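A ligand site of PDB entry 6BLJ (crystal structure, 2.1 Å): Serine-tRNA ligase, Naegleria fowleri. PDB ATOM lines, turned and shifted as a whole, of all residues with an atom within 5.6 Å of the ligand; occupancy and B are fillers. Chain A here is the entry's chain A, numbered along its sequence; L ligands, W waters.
NH1 of Arg 329 lies within salt-bridge range of OE1 of Glu 316, 3.0 Å away. The backbone carbonyl oxygen of Phe 328 is in hydrogen-bond range of the guanidinium group of Arg 450, at 2.9 Å. The backbone carbonyl oxygen (O) of Ser 409 lies within hydrogen-bond range of the backbone NH (N) of Thr 444 (3.0 Å). The side-chain amino group of Lys 335 sits at hydrogen-bond distance from the side-chain hydroxyl of Thr 283 (2.8 Å). ND1 of His 331 is in hydrogen-bond range of O of Arg 314 (2.8 Å). NH1 of Arg 450 is in salt-bridge range of OE2 of Glu 406 (3.1 Å).
Water W4 lies within hydrogen-bond range of OE2 of Glu 316, N2 of the ligand and NH1 of Arg 314. Water W2 lies within hydrogen-bond range of the side-chain hydroxyl (OG) of Ser 449 (2.8 Å), a nitrogen (N5) of the ligand (2.9 Å) and the backbone NH (N) of Arg 450 (2.9 Å).
Residues that only touch the ligand: Phe 328 (3.2 Å), Arg 329 (3.4 Å), Phe 333 (3.5 Å), Lys 335 (3.8 Å), Glu 406 (3.99 Å), Thr 444 (3.5 Å), Ala 447 (3.5 Å) and Arg 450 (3.6 Å). Of the 19 residues printed, 14 come within 4 Å of the ligand.
The side-chain carboxylate (OE2) of Glu 316 sits at hydrogen-bond distance from a nitrogen (N3) of the ligand. O of Val 330 sits at hydrogen-bond distance from N3 of the ligand (2.8 Å). The guanidinium group (NH2) of Arg 314 lies within salt-bridge range of an oxygen (O2) of the ligand (2.9 Å). O3 of the ligand sits at hydrogen-bond distance from OG of Ser 409 (2.6 Å). O6 of the ligand lies within hydrogen-bond range of N of Val 408 (3.3 Å). O of Leu 407 sits at hydrogen-bond distance from O7 of the ligand, 2.8 Å away. N of Val 330 is in hydrogen-bond range of N4 of the ligand.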
ATOM      1  N   THR A 283       3.669   7.392  19.232  1.00  0.00           N
ATOM      2  CA  THR A 283       3.593   6.039  18.696  1.00  0.00           C
ATOM      3  C   THR A 283       2.466   5.303  19.431  1.00  0.00           C
ATOM      4  O   THR A 283       2.274   5.520  20.628  1.00  0.00           O
ATOM      5  CB  THR A 283       4.932   5.284  18.866  1.00  0.00           C
ATOM      6  OG1 THR A 283       4.749   3.882  18.623  1.00  0.00           O
ATOM      7  CG2 THR A 283       5.542   5.463  20.287  1.00  0.00           C
ATOM      8  N   ARG A 314       5.218  14.091  16.537  1.00  0.00           N
ATOM      9  CA  ARG A 314       6.551  14.251  17.093  1.00  0.00           C
ATOM     10  C   ARG A 314       7.068  15.655  16.834  1.00  0.00           C
ATOM     11  O   ARG A 314       7.100  16.106  15.692  1.00  0.00           O
ATOM     12  CB  ARG A 314       7.496  13.202  16.509  1.00  0.00           C
ATOM     13  CG  ARG A 314       7.047  11.792  16.830  1.00  0.00           C
ATOM     14  CD  ARG A 314       8.104  10.810  16.539  1.00  0.00           C
ATOM     15  NE  ARG A 314       7.638   9.457  16.797  1.00  0.00           N
ATOM     16  CZ  ARG A 314       8.459   8.422  16.879  1.00  0.00           C
ATOM     17  NH1 ARG A 314       9.773   8.612  16.732  1.00  0.00           N
ATOM     18  NH2 ARG A 314       7.964   7.212  17.080  1.00  0.00           N
ATOM     19  N   GLU A 316      10.123  16.734  17.088  1.00  0.00           N
ATOM     20  CA  GLU A 316      11.417  16.707  16.371  1.00  0.00           C
ATOM     21  C   GLU A 316      12.272  17.923  16.721  1.00  0.00           C
ATOM     22  O   GLU A 316      12.982  18.478  15.875  1.00  0.00           O
ATOM     23  CB  GLU A 316      11.207  16.616  14.852  1.00  0.00           C
ATOM     24  CG  GLU A 316      10.473  15.343  14.406  1.00  0.00           C
ATOM     25  CD  GLU A 316      11.291  14.113  14.684  1.00  0.00           C
ATOM     26  OE1 GLU A 316      12.522  14.195  14.499  1.00  0.00           O
ATOM     27  OE2 GLU A 316      10.713  13.064  15.072  1.00  0.00           O
ATOM     28  N   ILE A 327       8.340  14.362   3.020  1.00  0.00           N
ATOM     29  CA  ILE A 327       7.601  13.765   4.122  1.00  0.00           C
ATOM     30  C   ILE A 327       8.361  12.601   4.767  1.00  0.00           C
ATOM     31  O   ILE A 327       7.755  11.724   5.395  1.00  0.00           O
ATOM     32  CB  ILE A 327       6.187  13.366   3.666  1.00  0.00           C
ATOM     33  CG1 ILE A 327       6.210  12.205   2.649  1.00  0.00           C
ATOM     34  CG2 ILE A 327       5.491  14.593   3.035  1.00  0.00           C
ATOM     35  CD1 ILE A 327       4.766  11.805   2.199  1.00  0.00           C
ATOM     36  N   PHE A 328       9.691  12.583   4.609  1.00  0.00           N
ATOM     37  CA  PHE A 328      10.534  11.583   5.263  1.00  0.00           C
ATOM     38  C   PHE A 328      10.567  11.781   6.786  1.00  0.00           C
ATOM     39  O   PHE A 328      10.503  10.811   7.550  1.00  0.00           O
ATOM     40  CB  PHE A 328      11.939  11.659   4.671  1.00  0.00           C
ATOM     41  CG  PHE A 328      12.932  10.725   5.293  1.00  0.00           C
ATOM     42  CD1 PHE A 328      13.621  11.093   6.447  1.00  0.00           C
ATOM     43  CD2 PHE A 328      13.228   9.502   4.704  1.00  0.00           C
ATOM     44  CE1 PHE A 328      14.566  10.240   7.026  1.00  0.00           C
ATOM     45  CE2 PHE A 328      14.183   8.646   5.263  1.00  0.00           C
ATOM     46  CZ  PHE A 328      14.842   9.012   6.422  1.00  0.00           C
ATOM     47  N   ARG A 329      10.713  13.024   7.227  1.00  0.00           N
ATOM     48  CA  ARG A 329      10.697  13.360   8.647  1.00  0.00           C
ATOM     49  C   ARG A 329       9.697  14.487   8.834  1.00  0.00           C
ATOM     50  O   ARG A 329       9.958  15.632   8.433  1.00  0.00           O
ATOM     51  CB  ARG A 329      12.083  13.786   9.145  1.00  0.00           C
ATOM     52  CG  ARG A 329      12.107  14.144  10.628  1.00  0.00           C
ATOM     53  CD  ARG A 329      13.474  14.679  11.053  1.00  0.00           C
ATOM     54  NE  ARG A 329      14.534  13.714  10.787  1.00  0.00           N
ATOM     55  CZ  ARG A 329      14.857  12.702  11.588  1.00  0.00           C
ATOM     56  NH1 ARG A 329      14.202  12.523  12.733  1.00  0.00           N
ATOM     57  NH2 ARG A 329      15.839  11.874  11.255  1.00  0.00           N
ATOM     58  N   VAL A 330       8.569  14.175   9.485  1.00  0.00           N
ATOM     59  CA  VAL A 330       7.466  15.103   9.652  1.00  0.00           C
ATOM     60  C   VAL A 330       7.036  15.086  11.121  1.00  0.00           C
ATOM     61  O   VAL A 330       7.545  14.314  11.923  1.00  0.00           O
ATOM     62  CB  VAL A 330       6.283  14.758   8.719  1.00  0.00           C
ATOM     63  CG1 VAL A 330       6.642  15.083   7.264  1.00  0.00           C
ATOM     64  CG2 VAL A 330       5.920  13.274   8.852  1.00  0.00           C
ATOM     65  N   HIS A 331       6.083  15.971  11.461  1.00  0.00           N
ATOM     66  CA  HIS A 331       5.482  16.004  12.796  1.00  0.00           C
ATOM     67  C   HIS A 331       4.264  15.111  12.921  1.00  0.00           C
ATOM     68  O   HIS A 331       3.812  14.879  14.048  1.00  0.00           O
ATOM     69  CB  HIS A 331       5.070  17.431  13.181  1.00  0.00           C
ATOM     70  CG  HIS A 331       6.190  18.419  13.185  1.00  0.00           C
ATOM     71  ND1 HIS A 331       7.274  18.307  14.023  1.00  0.00           N
ATOM     72  CD2 HIS A 331       6.381  19.552  12.469  1.00  0.00           C
ATOM     73  CE1 HIS A 331       8.094  19.332  13.817  1.00  0.00           C
ATOM     74  NE2 HIS A 331       7.578  20.091  12.876  1.00  0.00           N
ATOM     75  N   PHE A 333       2.338  11.540  11.136  1.00  0.00           N
ATOM     76  CA  PHE A 333       2.370  10.409  10.210  1.00  0.00           C
ATOM     77  C   PHE A 333       1.595   9.242  10.808  1.00  0.00           C
ATOM     78  O   PHE A 333       1.453   9.127  12.035  1.00  0.00           O
ATOM     79  CB  PHE A 333       3.825  10.017   9.878  1.00  0.00           C
ATOM     80  CG  PHE A 333       4.636   9.606  11.090  1.00  0.00           C
ATOM     81  CD1 PHE A 333       5.277  10.561  11.866  1.00  0.00           C
ATOM     82  CD2 PHE A 333       4.780   8.272  11.437  1.00  0.00           C
ATOM     83  CE1 PHE A 333       6.042  10.193  12.976  1.00  0.00           C
ATOM     84  CE2 PHE A 333       5.530   7.902  12.555  1.00  0.00           C
ATOM     85  CZ  PHE A 333       6.172   8.874  13.324  1.00  0.00           C
ATOM     86  N   LYS A 335       1.232   5.136  11.480  1.00  0.00           N
ATOM     87  CA  LYS A 335       2.160   4.033  11.680  1.00  0.00           C
ATOM     88  C   LYS A 335       1.403   2.803  12.164  1.00  0.00           C
ATOM     89  O   LYS A 335       0.561   2.872  13.061  1.00  0.00           O
ATOM     90  CB  LYS A 335       3.275   4.420  12.684  1.00  0.00           C
ATOM     91  CG  LYS A 335       4.283   3.267  12.918  1.00  0.00           C
ATOM     92  CD  LYS A 335       5.561   3.729  13.644  1.00  0.00           C
ATOM     93  CE  LYS A 335       5.310   4.298  15.053  1.00  0.00           C
ATOM     94  NZ  LYS A 335       4.500   3.404  15.922  1.00  0.00           N
ATOM     95  N   LYS A 388      18.084  -3.732  20.251  1.00  0.00           N
ATOM     96  CA  LYS A 388      17.302  -3.075  19.211  1.00  0.00           C
ATOM     97  C   LYS A 388      17.876  -3.413  17.845  1.00  0.00           C
ATOM     98  O   LYS A 388      19.087  -3.264  17.620  1.00  0.00           O
ATOM     99  CB  LYS A 388      17.265  -1.551  19.422  1.00  0.00           C
ATOM    100  CG  LYS A 388      16.416  -0.751  18.423  1.00  0.00           C
ATOM    101  CD  LYS A 388      16.032   0.595  19.013  1.00  0.00           C
ATOM    102  CE  LYS A 388      16.785   1.731  18.363  1.00  0.00           C
ATOM    103  NZ  LYS A 388      16.246   2.095  17.010  1.00  0.00           N
ATOM    104  N   GLU A 406      16.707   4.309   8.158  1.00  0.00           N
ATOM    105  CA  GLU A 406      15.840   3.501   8.995  1.00  0.00           C
ATOM    106  C   GLU A 406      14.367   3.672   8.612  1.00  0.00           C
ATOM    107  O   GLU A 406      13.870   4.793   8.407  1.00  0.00           O
ATOM    108  CB  GLU A 406      16.057   3.852  10.479  1.00  0.00           C
ATOM    109  CG  GLU A 406      15.530   5.206  10.932  1.00  0.00           C
ATOM    110  CD  GLU A 406      16.416   6.389  10.533  1.00  0.00           C
ATOM    111  OE1 GLU A 406      17.429   6.184   9.833  1.00  0.00           O
ATOM    112  OE2 GLU A 406      16.072   7.534  10.921  1.00  0.00           O
ATOM    113  N   LEU A 407      13.680   2.541   8.475  1.00  0.00           N
ATOM    114  CA  LEU A 407      12.222   2.464   8.300  1.00  0.00           C
ATOM    115  C   LEU A 407      11.539   1.793   9.479  1.00  0.00           C
ATOM    116  O   LEU A 407      10.329   2.012   9.681  1.00  0.00           O
ATOM    117  CB  LEU A 407      11.850   1.642   7.050  1.00  0.00           C
ATOM    118  CG  LEU A 407      11.958   2.249   5.655  1.00  0.00           C
ATOM    119  CD1 LEU A 407      11.231   1.375   4.633  1.00  0.00           C
ATOM    120  CD2 LEU A 407      11.369   3.631   5.709  1.00  0.00           C
ATOM    121  N   VAL A 408      12.271   0.962  10.223  1.00  0.00           N
ATOM    122  CA  VAL A 408      11.735   0.090  11.259  1.00  0.00           C
ATOM    123  C   VAL A 408      12.711   0.067  12.419  1.00  0.00           C
ATOM    124  O   VAL A 408      13.927   0.009  12.211  1.00  0.00           O
ATOM    125  CB  VAL A 408      11.505  -1.344  10.730  1.00  0.00           C
ATOM    126  CG1 VAL A 408      11.332  -2.341  11.885  1.00  0.00           C
ATOM    127  CG2 VAL A 408      10.313  -1.388   9.778  1.00  0.00           C
ATOM    128  N   SER A 409      12.195   0.132  13.642  1.00  0.00           N
ATOM    129  CA  SER A 409      12.940  -0.218  14.835  1.00  0.00           C
ATOM    130  C   SER A 409      12.177  -1.299  15.600  1.00  0.00           C
ATOM    131  O   SER A 409      10.938  -1.258  15.685  1.00  0.00           O
ATOM    132  CB  SER A 409      13.185   1.017  15.718  1.00  0.00           C
ATOM    133  OG  SER A 409      11.935   1.507  16.169  1.00  0.00           O
ATOM    134  N   THR A 444       8.070  -1.419  14.740  1.00  0.00           N
ATOM    135  CA  THR A 444       7.401  -0.869  13.561  1.00  0.00           C
ATOM    136  C   THR A 444       7.045  -1.984  12.593  1.00  0.00           C
ATOM    137  O   THR A 444       7.829  -2.901  12.362  1.00  0.00           O
ATOM    138  CB  THR A 444       8.308   0.099  12.818  1.00  0.00           C
ATOM    139  OG1 THR A 444       9.077   0.881  13.734  1.00  0.00           O
ATOM    140  CG2 THR A 444       7.476   0.984  11.861  1.00  0.00           C
ATOM    141  N   ALA A 447       5.646   2.874   8.988  1.00  0.00           N
ATOM    142  CA  ALA A 447       5.290   4.272   9.107  1.00  0.00           C
ATOM    143  C   ALA A 447       5.114   4.799   7.676  1.00  0.00           C
ATOM    144  O   ALA A 447       6.068   4.778   6.892  1.00  0.00           O
ATOM    145  CB  ALA A 447       6.381   5.040   9.857  1.00  0.00           C
ATOM    146  N   SER A 449       4.331   7.561   5.704  1.00  0.00           N
ATOM    147  CA  SER A 449       4.892   8.655   4.908  1.00  0.00           C
ATOM    148  C   SER A 449       6.330   8.364   4.480  1.00  0.00           C
ATOM    149  O   SER A 449       6.701   8.573   3.323  1.00  0.00           O
ATOM    150  CB  SER A 449       4.769  10.000   5.646  1.00  0.00           C
ATOM    151  OG  SER A 449       5.774  10.209   6.633  1.00  0.00           O
ATOM    152  N   ARG A 450       7.144   7.814   5.393  1.00  0.00           N
ATOM    153  CA  ARG A 450       8.513   7.452   5.021  1.00  0.00           C
ATOM    154  C   ARG A 450       8.558   6.207   4.124  1.00  0.00           C
ATOM    155  O   ARG A 450       9.430   6.096   3.254  1.00  0.00           O
ATOM    156  CB  ARG A 450       9.374   7.241   6.276  1.00  0.00           C
ATOM    157  CG  ARG A 450      10.883   7.052   6.007  1.00  0.00           C
ATOM    158  CD  ARG A 450      11.691   6.970   7.302  1.00  0.00           C
ATOM    159  NE  ARG A 450      11.644   8.234   8.046  1.00  0.00           N
ATOM    160  CZ  ARG A 450      12.393   8.483   9.112  1.00  0.00           C
ATOM    161  NH1 ARG A 450      13.258   7.557   9.558  1.00  0.00           N
ATOM    162  NH2 ARG A 450      12.302   9.668   9.718  1.00  0.00           N
HETATM  163  P1  LIG L   1      11.033   5.265  16.407  1.00  0.00           P
HETATM  164  O1  LIG L   1      11.840   6.551  16.629  1.00  0.00           O
HETATM  165  O2  LIG L   1       9.816   5.041  17.217  1.00  0.00           O
HETATM  166  O3  LIG L   1      11.992   4.087  16.451  1.00  0.00           O
HETATM  167  O4  LIG L   1      10.540   5.345  14.896  1.00  0.00           O
HETATM  168  C1  LIG L   1       9.877   4.247  14.273  1.00  0.00           C
HETATM  169  C2  LIG L   1       9.722   4.490  12.784  1.00  0.00           C
HETATM  170  O5  LIG L   1       8.761   5.562  12.561  1.00  0.00           O
HETATM  171  C3  LIG L   1      10.966   4.961  12.074  1.00  0.00           C
HETATM  172  O6  LIG L   1      11.830   3.891  11.720  1.00  0.00           O
HETATM  173  C4  LIG L   1      10.421   5.718  10.878  1.00  0.00           C
HETATM  174  O7  LIG L   1      10.029   4.807   9.865  1.00  0.00           O
HETATM  175  C5  LIG L   1       9.168   6.352  11.464  1.00  0.00           C
HETATM  176  N1  LIG L   1       9.378   7.741  11.938  1.00  0.00           N
HETATM  177  C6  LIG L   1       9.982   8.109  13.119  1.00  0.00           C
HETATM  178  N2  LIG L   1      10.046   9.411  13.289  1.00  0.00           N
HETATM  179  C7  LIG L   1       9.438   9.934  12.167  1.00  0.00           C
HETATM  180  C8  LIG L   1       9.177  11.255  11.745  1.00  0.00           C
HETATM  181  N3  LIG L   1       9.472  12.351  12.471  1.00  0.00           N
HETATM  182  N4  LIG L   1       8.586  11.421  10.538  1.00  0.00           N
HETATM  183  C9  LIG L   1       8.239  10.343   9.828  1.00  0.00           C
HETATM  184  N5  LIG L   1       8.412   9.054  10.138  1.00  0.00           N
HETATM  185  C10 LIG L   1       9.024   8.910  11.312  1.00  0.00           C
HETATM  186  O   HOH W   1      13.238   7.825  18.653  1.00  0.00           O
HETATM  187  O   HOH W   2       6.469   8.023   8.249  1.00  0.00           O
HETATM  188  O   HOH W   3      13.461   7.117  14.655  1.00  0.00           O
HETATM  189  O   HOH W   4      11.720  10.544  15.133  1.00  0.00           O
